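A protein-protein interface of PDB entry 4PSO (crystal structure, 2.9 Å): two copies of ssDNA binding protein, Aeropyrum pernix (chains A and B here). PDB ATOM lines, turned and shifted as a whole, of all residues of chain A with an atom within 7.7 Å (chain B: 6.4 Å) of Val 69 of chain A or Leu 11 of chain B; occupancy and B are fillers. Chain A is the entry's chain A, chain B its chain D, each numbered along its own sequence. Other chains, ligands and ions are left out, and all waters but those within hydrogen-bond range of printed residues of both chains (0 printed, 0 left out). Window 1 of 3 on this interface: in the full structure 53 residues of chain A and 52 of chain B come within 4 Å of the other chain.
Leu 11 of chain A touches Val 12 of chain B, and with the chains exchanged Val 12 of chain A touches Leu 11 of chain B.
Val 69 of chain A touches Trp 95 of chain B, and with the chains exchanged Trp 95 of chain A touches Val 69 of chain B.
Trp 95 of chain A touches Ile 13 of chain B, but with the chains exchanged Ile 13 of chain A does not touch Trp 95 of chain B (4.03 Å).
Trp 95 of chain B touches its own counterpart, Trp 95 of chain A.
Printed residues of chain B that touch a printed residue of chain A: Leu 11, Val 12, Ile 13, Val 69 and Trp 95.
Hydrophobic or aromatic side chains of chain B within 4 Å of the printed part of chain A: Leu 11, Ile 13, Val 69 and Trp 95.
Printed residues of chain A that touch a printed residue of chain B: Leu 11, Val 12, Ile 13, Leu 67, Asp 68, Val 69, Trp 95, Arg 96 and Arg 97.
Hydrophobic or aromatic side chains of chain A within 4 Å of the printed part of chain B: Leu 11, Ile 13, Val 69 and Trp 95.
Among the printed residues, 15 pairs touch across the chains.
Ala 15 of chain A touches none of the printed residues of chain B.
Of the printed residues of chain B, Asp 68 of chain A touches Trp 95 (3.9 Å).
Arg 71 of chain A touches none of the printed residues of chain B.
Printed residues of chain B within 4 Å of Arg 96 of chain A: Trp 95 (3.3 Å).
Of the printed residues of chain B, Arg 97 of chain A touches Trp 95 (3.5 Å).
No residue of chain A comes within 4 Å of Gly 10 of chain B.
Printed residues of chain A within 4 Å of Leu 11 of chain B: Leu 11, Val 12, Ile 13 and Val 69.
Among the printed residues, merely in contact across the chains: Leu 11 of chain A with Leu 11 of chain B (3.995 Å), Leu 11 of chain A with Val 12 of chain B (3.9 Å), Leu 11 of chain A with Ile 13 of chain B (3.8 Å), Leu 11 of chain A with Val 69 of chain B (3.7 Å), Val 12 of chain A with Leu 11 of chain B (3.9 Å), Ile 13 of chain A with Leu 11 of chain B (3.8 Å), Asp 68 of chain A with Trp 95 of chain B (3.9 Å), Val 69 of chain A with Leu 11 of chain B (3.9 Å), Val 69 of chain A with Trp 95 of chain B (3.7 Å), Trp 95 of chain A with Ile 13 of chain B (3.9 Å), Trp 95 of chain A with Val 69 of chain B (3.5 Å), Trp 95 of chain A with Trp 95 of chain B (3.4 Å), Arg 96 of chain A with Trp 95 of chain B (3.3 Å) and Arg 97 of chain A with Trp 95 of chain B (3.5 Å).
O of Leu 67 of chain A is in hydrogen-bond range of NE1 of Trp 95 of chain B.
The backbone carbonyl oxygen (O) of Val 12 of chain A sits at hydrogen-bond distance from the backbone NH (N) of Val 70 of chain A, 2.9 Å away.
The backbone carbonyl oxygen (O) of Asp 68 of chain A lies within hydrogen-bond range of the backbone NH (N) of Ala 14 of chain A.
N of Asp 65 of chain A sits at hydrogen-bond distance from OD2 of Asp 68 of chain A, 3.1 Å away.
The side-chain carboxylate (OD1) of Asp 68 of chain A lies within hydrogen-bond range of the backbone NH (N) of Arg 97 of chain A (2.8 Å).
The backbone NH (N) of Val 70 of chain B lies within hydrogen-bond range of the backbone carbonyl oxygen (O) of Val 12 of chain B (2.9 Å).
The backbone carbonyl oxygen of Val 69 of chain B sits at hydrogen-bond distance from the backbone NH of Trp 95 of chain B, at 2.7 Å.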
ATOM      1  N   GLY A  10     -30.281   7.250 -27.593  1.00  0.00           N
ATOM      2  CA  GLY A  10     -30.550   7.025 -26.188  1.00  0.00           C
ATOM      3  C   GLY A  10     -29.218   6.754 -25.520  1.00  0.00           C
ATOM      4  O   GLY A  10     -28.170   6.982 -26.121  1.00  0.00           O
ATOM      5  N   LEU A  11     -29.242   6.282 -24.279  1.00  0.00           N
ATOM      6  CA  LEU A  11     -28.004   5.949 -23.584  1.00  0.00           C
ATOM      7  C   LEU A  11     -27.362   4.689 -24.165  1.00  0.00           C
ATOM      8  O   LEU A  11     -28.024   3.660 -24.334  1.00  0.00           O
ATOM      9  CB  LEU A  11     -28.256   5.773 -22.085  1.00  0.00           C
ATOM     10  CG  LEU A  11     -28.805   7.000 -21.354  1.00  0.00           C
ATOM     11  CD1 LEU A  11     -28.895   6.753 -19.859  1.00  0.00           C
ATOM     12  CD2 LEU A  11     -27.926   8.202 -21.639  1.00  0.00           C
ATOM     13  N   VAL A  12     -26.074   4.782 -24.490  1.00  0.00           N
ATOM     14  CA  VAL A  12     -25.335   3.641 -25.019  1.00  0.00           C
ATOM     15  C   VAL A  12     -23.847   3.740 -24.661  1.00  0.00           C
ATOM     16  O   VAL A  12     -23.277   4.835 -24.618  1.00  0.00           O
ATOM     17  CB  VAL A  12     -25.514   3.517 -26.562  1.00  0.00           C
ATOM     18  CG1 VAL A  12     -24.940   4.734 -27.286  1.00  0.00           C
ATOM     19  CG2 VAL A  12     -24.890   2.230 -27.086  1.00  0.00           C
ATOM     20  N   ILE A  13     -23.237   2.594 -24.368  1.00  0.00           N
ATOM     21  CA  ILE A  13     -21.797   2.520 -24.136  1.00  0.00           C
ATOM     22  C   ILE A  13     -21.054   2.905 -25.410  1.00  0.00           C
ATOM     23  O   ILE A  13     -21.422   2.465 -26.502  1.00  0.00           O
ATOM     24  CB  ILE A  13     -21.368   1.112 -23.675  1.00  0.00           C
ATOM     25  CG1 ILE A  13     -22.101   0.735 -22.386  1.00  0.00           C
ATOM     26  CG2 ILE A  13     -19.860   1.050 -23.461  1.00  0.00           C
ATOM     27  CD1 ILE A  13     -21.613   1.493 -21.158  1.00  0.00           C
ATOM     28  N   ALA A  14     -20.029   3.742 -25.269  1.00  0.00           N
ATOM     29  CA  ALA A  14     -19.315   4.305 -26.413  1.00  0.00           C
ATOM     30  C   ALA A  14     -18.805   3.243 -27.376  1.00  0.00           C
ATOM     31  O   ALA A  14     -18.708   3.484 -28.577  1.00  0.00           O
ATOM     32  CB  ALA A  14     -18.159   5.162 -25.935  1.00  0.00           C
ATOM     33  N   ALA A  15     -18.503   2.064 -26.848  1.00  0.00           N
ATOM     34  CA  ALA A  15     -17.978   0.980 -27.660  1.00  0.00           C
ATOM     35  C   ALA A  15     -19.012   0.464 -28.654  1.00  0.00           C
ATOM     36  O   ALA A  15     -18.659  -0.156 -29.660  1.00  0.00           O
ATOM     37  CB  ALA A  15     -17.505  -0.149 -26.769  1.00  0.00           C
ATOM     38  N   LEU A  58     -15.795  11.486 -31.168  1.00  0.00           N
ATOM     39  CA  LEU A  58     -15.811  10.841 -29.860  1.00  0.00           C
ATOM     40  C   LEU A  58     -14.417  10.454 -29.369  1.00  0.00           C
ATOM     41  O   LEU A  58     -14.077  10.694 -28.210  1.00  0.00           O
ATOM     42  CB  LEU A  58     -16.717   9.605 -29.887  1.00  0.00           C
ATOM     43  CG  LEU A  58     -18.204   9.868 -30.145  1.00  0.00           C
ATOM     44  CD1 LEU A  58     -19.007   8.571 -30.171  1.00  0.00           C
ATOM     45  CD2 LEU A  58     -18.762  10.821 -29.099  1.00  0.00           C
ATOM     46  N   ALA A  64     -13.179  10.397 -25.621  1.00  0.00           N
ATOM     47  CA  ALA A  64     -14.023   9.509 -24.830  1.00  0.00           C
ATOM     48  C   ALA A  64     -13.481   8.083 -24.808  1.00  0.00           C
ATOM     49  O   ALA A  64     -13.119   7.536 -25.851  1.00  0.00           O
ATOM     50  CB  ALA A  64     -15.447   9.520 -25.369  1.00  0.00           C
ATOM     51  N   ASP A  65     -13.423   7.485 -23.621  1.00  0.00           N
ATOM     52  CA  ASP A  65     -13.040   6.082 -23.502  1.00  0.00           C
ATOM     53  C   ASP A  65     -14.214   5.218 -23.946  1.00  0.00           C
ATOM     54  O   ASP A  65     -15.366   5.646 -23.872  1.00  0.00           O
ATOM     55  CB  ASP A  65     -12.622   5.739 -22.069  1.00  0.00           C
ATOM     56  CG  ASP A  65     -12.068   4.329 -21.945  1.00  0.00           C
ATOM     57  OD1 ASP A  65     -11.300   3.906 -22.840  1.00  0.00           O
ATOM     58  OD2 ASP A  65     -12.400   3.641 -20.956  1.00  0.00           O
ATOM     59  N   LYS A  66     -13.929   4.007 -24.413  1.00  0.00           N
ATOM     60  CA  LYS A  66     -14.979   3.146 -24.947  1.00  0.00           C
ATOM     61  C   LYS A  66     -15.901   2.575 -23.877  1.00  0.00           C
ATOM     62  O   LYS A  66     -16.898   1.929 -24.200  1.00  0.00           O
ATOM     63  CB  LYS A  66     -14.380   2.000 -25.765  1.00  0.00           C
ATOM     64  CG  LYS A  66     -13.327   1.166 -25.056  1.00  0.00           C
ATOM     65  CD  LYS A  66     -12.849   0.058 -25.988  1.00  0.00           C
ATOM     66  CE  LYS A  66     -12.441   0.617 -27.348  1.00  0.00           C
ATOM     67  NZ  LYS A  66     -12.237  -0.453 -28.366  1.00  0.00           N
ATOM     68  N   LEU A  67     -15.576   2.801 -22.610  1.00  0.00           N
ATOM     69  CA  LEU A  67     -16.418   2.302 -21.531  1.00  0.00           C
ATOM     70  C   LEU A  67     -17.266   3.428 -20.948  1.00  0.00           C
ATOM     71  O   LEU A  67     -17.958   3.245 -19.947  1.00  0.00           O
ATOM     72  CB  LEU A  67     -15.565   1.650 -20.439  1.00  0.00           C
ATOM     73  CG  LEU A  67     -14.967   0.280 -20.792  1.00  0.00           C
ATOM     74  CD1 LEU A  67     -14.297  -0.367 -19.586  1.00  0.00           C
ATOM     75  CD2 LEU A  67     -16.021  -0.641 -21.382  1.00  0.00           C
ATOM     76  N   ASP A  68     -17.200   4.596 -21.579  1.00  0.00           N
ATOM     77  CA  ASP A  68     -18.043   5.725 -21.199  1.00  0.00           C
ATOM     78  C   ASP A  68     -19.427   5.601 -21.833  1.00  0.00           C
ATOM     79  O   ASP A  68     -19.683   4.675 -22.606  1.00  0.00           O
ATOM     80  CB  ASP A  68     -17.387   7.050 -21.603  1.00  0.00           C
ATOM     81  CG  ASP A  68     -16.138   7.351 -20.797  1.00  0.00           C
ATOM     82  OD1 ASP A  68     -15.994   6.783 -19.695  1.00  0.00           O
ATOM     83  OD2 ASP A  68     -15.301   8.158 -21.262  1.00  0.00           O
ATOM     84  N   VAL A  69     -20.318   6.533 -21.507  1.00  0.00           N
ATOM     85  CA  VAL A  69     -21.673   6.519 -22.052  1.00  0.00           C
ATOM     86  C   VAL A  69     -21.939   7.778 -22.871  1.00  0.00           C
ATOM     87  O   VAL A  69     -21.672   8.892 -22.417  1.00  0.00           O
ATOM     88  CB  VAL A  69     -22.737   6.392 -20.929  1.00  0.00           C
ATOM     89  CG1 VAL A  69     -24.141   6.633 -21.474  1.00  0.00           C
ATOM     90  CG2 VAL A  69     -22.653   5.025 -20.270  1.00  0.00           C
ATOM     91  N   VAL A  70     -22.455   7.603 -24.084  1.00  0.00           N
ATOM     92  CA  VAL A  70     -22.777   8.742 -24.935  1.00  0.00           C
ATOM     93  C   VAL A  70     -24.252   8.748 -25.327  1.00  0.00           C
ATOM     94  O   VAL A  70     -24.923   7.714 -25.295  1.00  0.00           O
ATOM     95  CB  VAL A  70     -21.922   8.756 -26.225  1.00  0.00           C
ATOM     96  CG1 VAL A  70     -20.449   8.895 -25.892  1.00  0.00           C
ATOM     97  CG2 VAL A  70     -22.174   7.497 -27.047  1.00  0.00           C
ATOM     98  N   ARG A  71     -24.752   9.922 -25.691  1.00  0.00           N
ATOM     99  CA  ARG A  71     -26.089  10.040 -26.256  1.00  0.00           C
ATOM    100  C   ARG A  71     -26.042  10.985 -27.444  1.00  0.00           C
ATOM    101  O   ARG A  71     -25.674  12.155 -27.322  1.00  0.00           O
ATOM    102  CB  ARG A  71     -27.098  10.519 -25.207  1.00  0.00           C
ATOM    103  CG  ARG A  71     -28.540  10.548 -25.712  1.00  0.00           C
ATOM    104  CD  ARG A  71     -29.541  10.520 -24.570  1.00  0.00           C
ATOM    105  NE  ARG A  71     -29.407  11.668 -23.676  1.00  0.00           N
ATOM    106  CZ  ARG A  71     -30.125  11.839 -22.571  1.00  0.00           C
ATOM    107  NH1 ARG A  71     -29.936  12.908 -21.811  1.00  0.00           N
ATOM    108  NH2 ARG A  71     -31.034  10.938 -22.227  1.00  0.00           N
ATOM    109  N   VAL A  92     -24.335  15.848 -28.983  1.00  0.00           N
ATOM    110  CA  VAL A  92     -23.678  14.716 -28.347  1.00  0.00           C
ATOM    111  C   VAL A  92     -23.534  14.943 -26.849  1.00  0.00           C
ATOM    112  O   VAL A  92     -23.000  15.963 -26.413  1.00  0.00           O
ATOM    113  CB  VAL A  92     -22.287  14.449 -28.965  1.00  0.00           C
ATOM    114  CG1 VAL A  92     -21.532  13.409 -28.157  1.00  0.00           C
ATOM    115  CG2 VAL A  92     -22.431  13.990 -30.405  1.00  0.00           C
ATOM    116  N   GLU A  93     -24.026  13.989 -26.065  1.00  0.00           N
ATOM    117  CA  GLU A  93     -23.887  14.044 -24.616  1.00  0.00           C
ATOM    118  C   GLU A  93     -22.886  12.984 -24.185  1.00  0.00           C
ATOM    119  O   GLU A  93     -22.814  11.913 -24.789  1.00  0.00           O
ATOM    120  CB  GLU A  93     -25.234  13.820 -23.926  1.00  0.00           C
ATOM    121  CG  GLU A  93     -26.358  14.671 -24.488  1.00  0.00           C
ATOM    122  CD  GLU A  93     -27.703  14.334 -23.885  1.00  0.00           C
ATOM    123  OE1 GLU A  93     -28.667  14.155 -24.657  1.00  0.00           O
ATOM    124  OE2 GLU A  93     -27.797  14.254 -22.641  1.00  0.00           O
ATOM    125  N   LEU A  94     -22.103  13.285 -23.155  1.00  0.00           N
ATOM    126  CA  LEU A  94     -21.073  12.362 -22.697  1.00  0.00           C
ATOM    127  C   LEU A  94     -21.069  12.232 -21.182  1.00  0.00           C
ATOM    128  O   LEU A  94     -21.135  13.226 -20.457  1.00  0.00           O
ATOM    129  CB  LEU A  94     -19.688  12.805 -23.180  1.00  0.00           C
ATOM    130  CG  LEU A  94     -18.498  11.971 -22.692  1.00  0.00           C
ATOM    131  CD1 LEU A  94     -18.608  10.533 -23.185  1.00  0.00           C
ATOM    132  CD2 LEU A  94     -17.178  12.590 -23.132  1.00  0.00           C
ATOM    133  N   TRP A  95     -20.992  10.990 -20.721  1.00  0.00           N
ATOM    134  CA  TRP A  95     -20.840  10.679 -19.310  1.00  0.00           C
ATOM    135  C   TRP A  95     -19.552   9.887 -19.114  1.00  0.00           C
ATOM    136  O   TRP A  95     -19.347   8.856 -19.758  1.00  0.00           O
ATOM    137  CB  TRP A  95     -22.035   9.880 -18.790  1.00  0.00           C
ATOM    138  CG  TRP A  95     -23.322  10.629 -18.731  1.00  0.00           C
ATOM    139  CD1 TRP A  95     -23.859  11.237 -17.635  1.00  0.00           C
ATOM    140  CD2 TRP A  95     -24.250  10.835 -19.804  1.00  0.00           C
ATOM    141  NE1 TRP A  95     -25.061  11.818 -17.961  1.00  0.00           N
ATOM    142  CE2 TRP A  95     -25.325  11.586 -19.288  1.00  0.00           C
ATOM    143  CE3 TRP A  95     -24.277  10.465 -21.153  1.00  0.00           C
ATOM    144  CZ2 TRP A  95     -26.414  11.974 -20.070  1.00  0.00           C
ATOM    145  CZ3 TRP A  95     -25.358  10.852 -21.931  1.00  0.00           C
ATOM    146  CH2 TRP A  95     -26.412  11.597 -21.386  1.00  0.00           C
ATOM    147  N   ARG A  96     -18.678  10.373 -18.241  1.00  0.00           N
ATOM    148  CA  ARG A  96     -17.395   9.713 -18.027  1.00  0.00           C
ATOM    149  C   ARG A  96     -17.427   8.718 -16.876  1.00  0.00           C
ATOM    150  O   ARG A  96     -18.020   8.969 -15.824  1.00  0.00           O
ATOM    151  CB  ARG A  96     -16.276  10.733 -17.805  1.00  0.00           C
ATOM    152  CG  ARG A  96     -15.970  11.570 -19.035  1.00  0.00           C
ATOM    153  CD  ARG A  96     -14.739  12.435 -18.839  1.00  0.00           C
ATOM    154  NE  ARG A  96     -14.377  13.122 -20.075  1.00  0.00           N
ATOM    155  CZ  ARG A  96     -13.721  12.545 -21.078  1.00  0.00           C
ATOM    156  NH1 ARG A  96     -13.361  11.269 -20.993  1.00  0.00           N
ATOM    157  NH2 ARG A  96     -13.424  13.239 -22.167  1.00  0.00           N
ATOM    158  N   ARG A  97     -16.779   7.582 -17.113  1.00  0.00           N
ATOM    159  CA  ARG A  97     -16.792   6.438 -16.212  1.00  0.00           C
ATOM    160  C   ARG A  97     -16.062   6.689 -14.903  1.00  0.00           C
ATOM    161  O   ARG A  97     -14.942   7.200 -14.892  1.00  0.00           O
ATOM    162  CB  ARG A  97     -16.152   5.241 -16.921  1.00  0.00           C
ATOM    163  CG  ARG A  97     -15.992   3.990 -16.078  1.00  0.00           C
ATOM    164  CD  ARG A  97     -15.499   2.837 -16.935  1.00  0.00           C
ATOM    165  NE  ARG A  97     -15.052   1.719 -16.111  1.00  0.00           N
ATOM    166  CZ  ARG A  97     -13.794   1.567 -15.711  1.00  0.00           C
ATOM    167  NH1 ARG A  97     -13.448   0.531 -14.960  1.00  0.00           N
ATOM    168  NH2 ARG A  97     -12.877   2.453 -16.078  1.00  0.00           N
ATOM    169  N   THR B   9     -31.050  -2.870 -14.214  1.00  0.00           N
ATOM    170  CA  THR B   9     -31.667  -1.643 -14.707  1.00  0.00           C
ATOM    171  C   THR B   9     -31.185  -1.331 -16.112  1.00  0.00           C
ATOM    172  O   THR B   9     -31.915  -0.760 -16.922  1.00  0.00           O
ATOM    173  CB  THR B   9     -31.358  -0.430 -13.807  1.00  0.00           C
ATOM    174  OG1 THR B   9     -29.951  -0.148 -13.839  1.00  0.00           O
ATOM    175  CG2 THR B   9     -31.796  -0.700 -12.375  1.00  0.00           C
ATOM    176  N   GLY B  10     -29.949  -1.716 -16.402  1.00  0.00           N
ATOM    177  CA  GLY B  10     -29.313  -1.288 -17.630  1.00  0.00           C
ATOM    178  C   GLY B  10     -28.902   0.159 -17.442  1.00  0.00           C
ATOM    179  O   GLY B  10     -28.921   0.672 -16.321  1.00  0.00           O
ATOM    180  N   LEU B  11     -28.516   0.825 -18.522  1.00  0.00           N
ATOM    181  CA  LEU B  11     -28.136   2.226 -18.422  1.00  0.00           C
ATOM    182  C   LEU B  11     -29.371   3.086 -18.162  1.00  0.00           C
ATOM    183  O   LEU B  11     -30.370   2.984 -18.880  1.00  0.00           O
ATOM    184  CB  LEU B  11     -27.421   2.684 -19.693  1.00  0.00           C
ATOM    185  CG  LEU B  11     -26.140   1.926 -20.043  1.00  0.00           C
ATOM    186  CD1 LEU B  11     -25.449   2.553 -21.246  1.00  0.00           C
ATOM    187  CD2 LEU B  11     -25.212   1.895 -18.847  1.00  0.00           C
ATOM    188  N   VAL B  12     -29.307   3.930 -17.135  1.00  0.00           N
ATOM    189  CA  VAL B  12     -30.428   4.807 -16.818  1.00  0.00           C
ATOM    190  C   VAL B  12     -29.964   6.106 -16.158  1.00  0.00           C
ATOM    191  O   VAL B  12     -29.009   6.121 -15.373  1.00  0.00           O
ATOM    192  CB  VAL B  12     -31.459   4.092 -15.899  1.00  0.00           C
ATOM    193  CG1 VAL B  12     -30.844   3.758 -14.548  1.00  0.00           C
ATOM    194  CG2 VAL B  12     -32.715   4.937 -15.717  1.00  0.00           C
ATOM    195  N   ILE B  13     -30.633   7.203 -16.508  1.00  0.00           N
ATOM    196  CA  ILE B  13     -30.393   8.485 -15.862  1.00  0.00           C
ATOM    197  C   ILE B  13     -30.766   8.363 -14.387  1.00  0.00           C
ATOM    198  O   ILE B  13     -31.808   7.795 -14.048  1.00  0.00           O
ATOM    199  CB  ILE B  13     -31.195   9.617 -16.538  1.00  0.00           C
ATOM    200  CG1 ILE B  13     -30.773   9.755 -18.003  1.00  0.00           C
ATOM    201  CG2 ILE B  13     -30.961  10.939 -15.833  1.00  0.00           C
ATOM    202  CD1 ILE B  13     -29.394  10.370 -18.180  1.00  0.00           C
ATOM    203  N   LYS B  20     -37.382   2.615 -12.975  1.00  0.00           N
ATOM    204  CA  LYS B  20     -36.777   1.551 -13.776  1.00  0.00           C
ATOM    205  C   LYS B  20     -36.691   0.260 -12.975  1.00  0.00           C
ATOM    206  O   LYS B  20     -37.033  -0.816 -13.471  1.00  0.00           O
ATOM    207  CB  LYS B  20     -35.384   1.955 -14.269  1.00  0.00           C
ATOM    208  CG  LYS B  20     -34.789   0.993 -15.284  1.00  0.00           C
ATOM    209  CD  LYS B  20     -35.664   0.903 -16.526  1.00  0.00           C
ATOM    210  CE  LYS B  20     -34.881   0.400 -17.727  1.00  0.00           C
ATOM    211  NZ  LYS B  20     -35.671   0.549 -18.980  1.00  0.00           N
ATOM    212  N   VAL B  69     -25.415   9.087 -15.128  1.00  0.00           N
ATOM    213  CA  VAL B  69     -25.918   7.792 -15.571  1.00  0.00           C
ATOM    214  C   VAL B  69     -25.444   6.686 -14.635  1.00  0.00           C
ATOM    215  O   VAL B  69     -24.257   6.594 -14.318  1.00  0.00           O
ATOM    216  CB  VAL B  69     -25.478   7.474 -17.023  1.00  0.00           C
ATOM    217  CG1 VAL B  69     -25.798   6.029 -17.384  1.00  0.00           C
ATOM    218  CG2 VAL B  69     -26.152   8.427 -18.000  1.00  0.00           C
ATOM    219  N   VAL B  70     -26.378   5.856 -14.183  1.00  0.00           N
ATOM    220  CA  VAL B  70     -26.038   4.737 -13.314  1.00  0.00           C
ATOM    221  C   VAL B  70     -26.482   3.417 -13.933  1.00  0.00           C
ATOM    222  O   VAL B  70     -27.367   3.387 -14.789  1.00  0.00           O
ATOM    223  CB  VAL B  70     -26.689   4.872 -11.910  1.00  0.00           C
ATOM    224  CG1 VAL B  70     -26.180   6.113 -11.188  1.00  0.00           C
ATOM    225  CG2 VAL B  70     -28.207   4.895 -12.028  1.00  0.00           C
ATOM    226  N   ARG B  71     -25.850   2.329 -13.509  1.00  0.00           N
ATOM    227  CA  ARG B  71     -26.324   1.000 -13.868  1.00  0.00           C
ATOM    228  C   ARG B  71     -26.250   0.111 -12.639  1.00  0.00           C
ATOM    229  O   ARG B  71     -25.179  -0.094 -12.064  1.00  0.00           O
ATOM    230  CB  ARG B  71     -25.525   0.404 -15.023  1.00  0.00           C
ATOM    231  CG  ARG B  71     -26.095  -0.923 -15.509  1.00  0.00           C
ATOM    232  CD  ARG B  71     -25.637  -1.232 -16.915  1.00  0.00           C
ATOM    233  NE  ARG B  71     -24.185  -1.356 -16.997  1.00  0.00           N
ATOM    234  CZ  ARG B  71     -23.520  -1.549 -18.129  1.00  0.00           C
ATOM    235  NH1 ARG B  71     -22.199  -1.647 -18.115  1.00  0.00           N
ATOM    236  NH2 ARG B  71     -24.178  -1.633 -19.278  1.00  0.00           N
ATOM    237  N   GLU B  93     -22.756   0.844 -11.034  1.00  0.00           N
ATOM    238  CA  GLU B  93     -21.847   1.565 -11.917  1.00  0.00           C
ATOM    239  C   GLU B  93     -22.308   3.012 -12.055  1.00  0.00           C
ATOM    240  O   GLU B  93     -23.507   3.287 -12.050  1.00  0.00           O
ATOM    241  CB  GLU B  93     -21.775   0.890 -13.290  1.00  0.00           C
ATOM    242  CG  GLU B  93     -21.530  -0.614 -13.238  1.00  0.00           C
ATOM    243  CD  GLU B  93     -21.607  -1.269 -14.605  1.00  0.00           C
ATOM    244  OE1 GLU B  93     -22.295  -2.304 -14.732  1.00  0.00           O
ATOM    245  OE2 GLU B  93     -20.973  -0.758 -15.550  1.00  0.00           O
ATOM    246  N   TRP B  95     -21.618   6.907 -14.097  1.00  0.00           N
ATOM    247  CA  TRP B  95     -20.988   7.759 -15.098  1.00  0.00           C
ATOM    248  C   TRP B  95     -21.304   9.226 -14.816  1.00  0.00           C
ATOM    249  O   TRP B  95     -22.475   9.603 -14.740  1.00  0.00           O
ATOM    250  CB  TRP B  95     -21.451   7.374 -16.505  1.00  0.00           C
ATOM    251  CG  TRP B  95     -20.975   6.034 -16.971  1.00  0.00           C
ATOM    252  CD1 TRP B  95     -19.892   5.784 -17.758  1.00  0.00           C
ATOM    253  CD2 TRP B  95     -21.572   4.758 -16.693  1.00  0.00           C
ATOM    254  NE1 TRP B  95     -19.772   4.435 -17.985  1.00  0.00           N
ATOM    255  CE2 TRP B  95     -20.792   3.782 -17.341  1.00  0.00           C
ATOM    256  CE3 TRP B  95     -22.690   4.348 -15.961  1.00  0.00           C
ATOM    257  CZ2 TRP B  95     -21.089   2.421 -17.275  1.00  0.00           C
ATOM    258  CZ3 TRP B  95     -22.985   2.994 -15.898  1.00  0.00           C
ATOM    259  CH2 TRP B  95     -22.188   2.049 -16.551  1.00  0.00           C
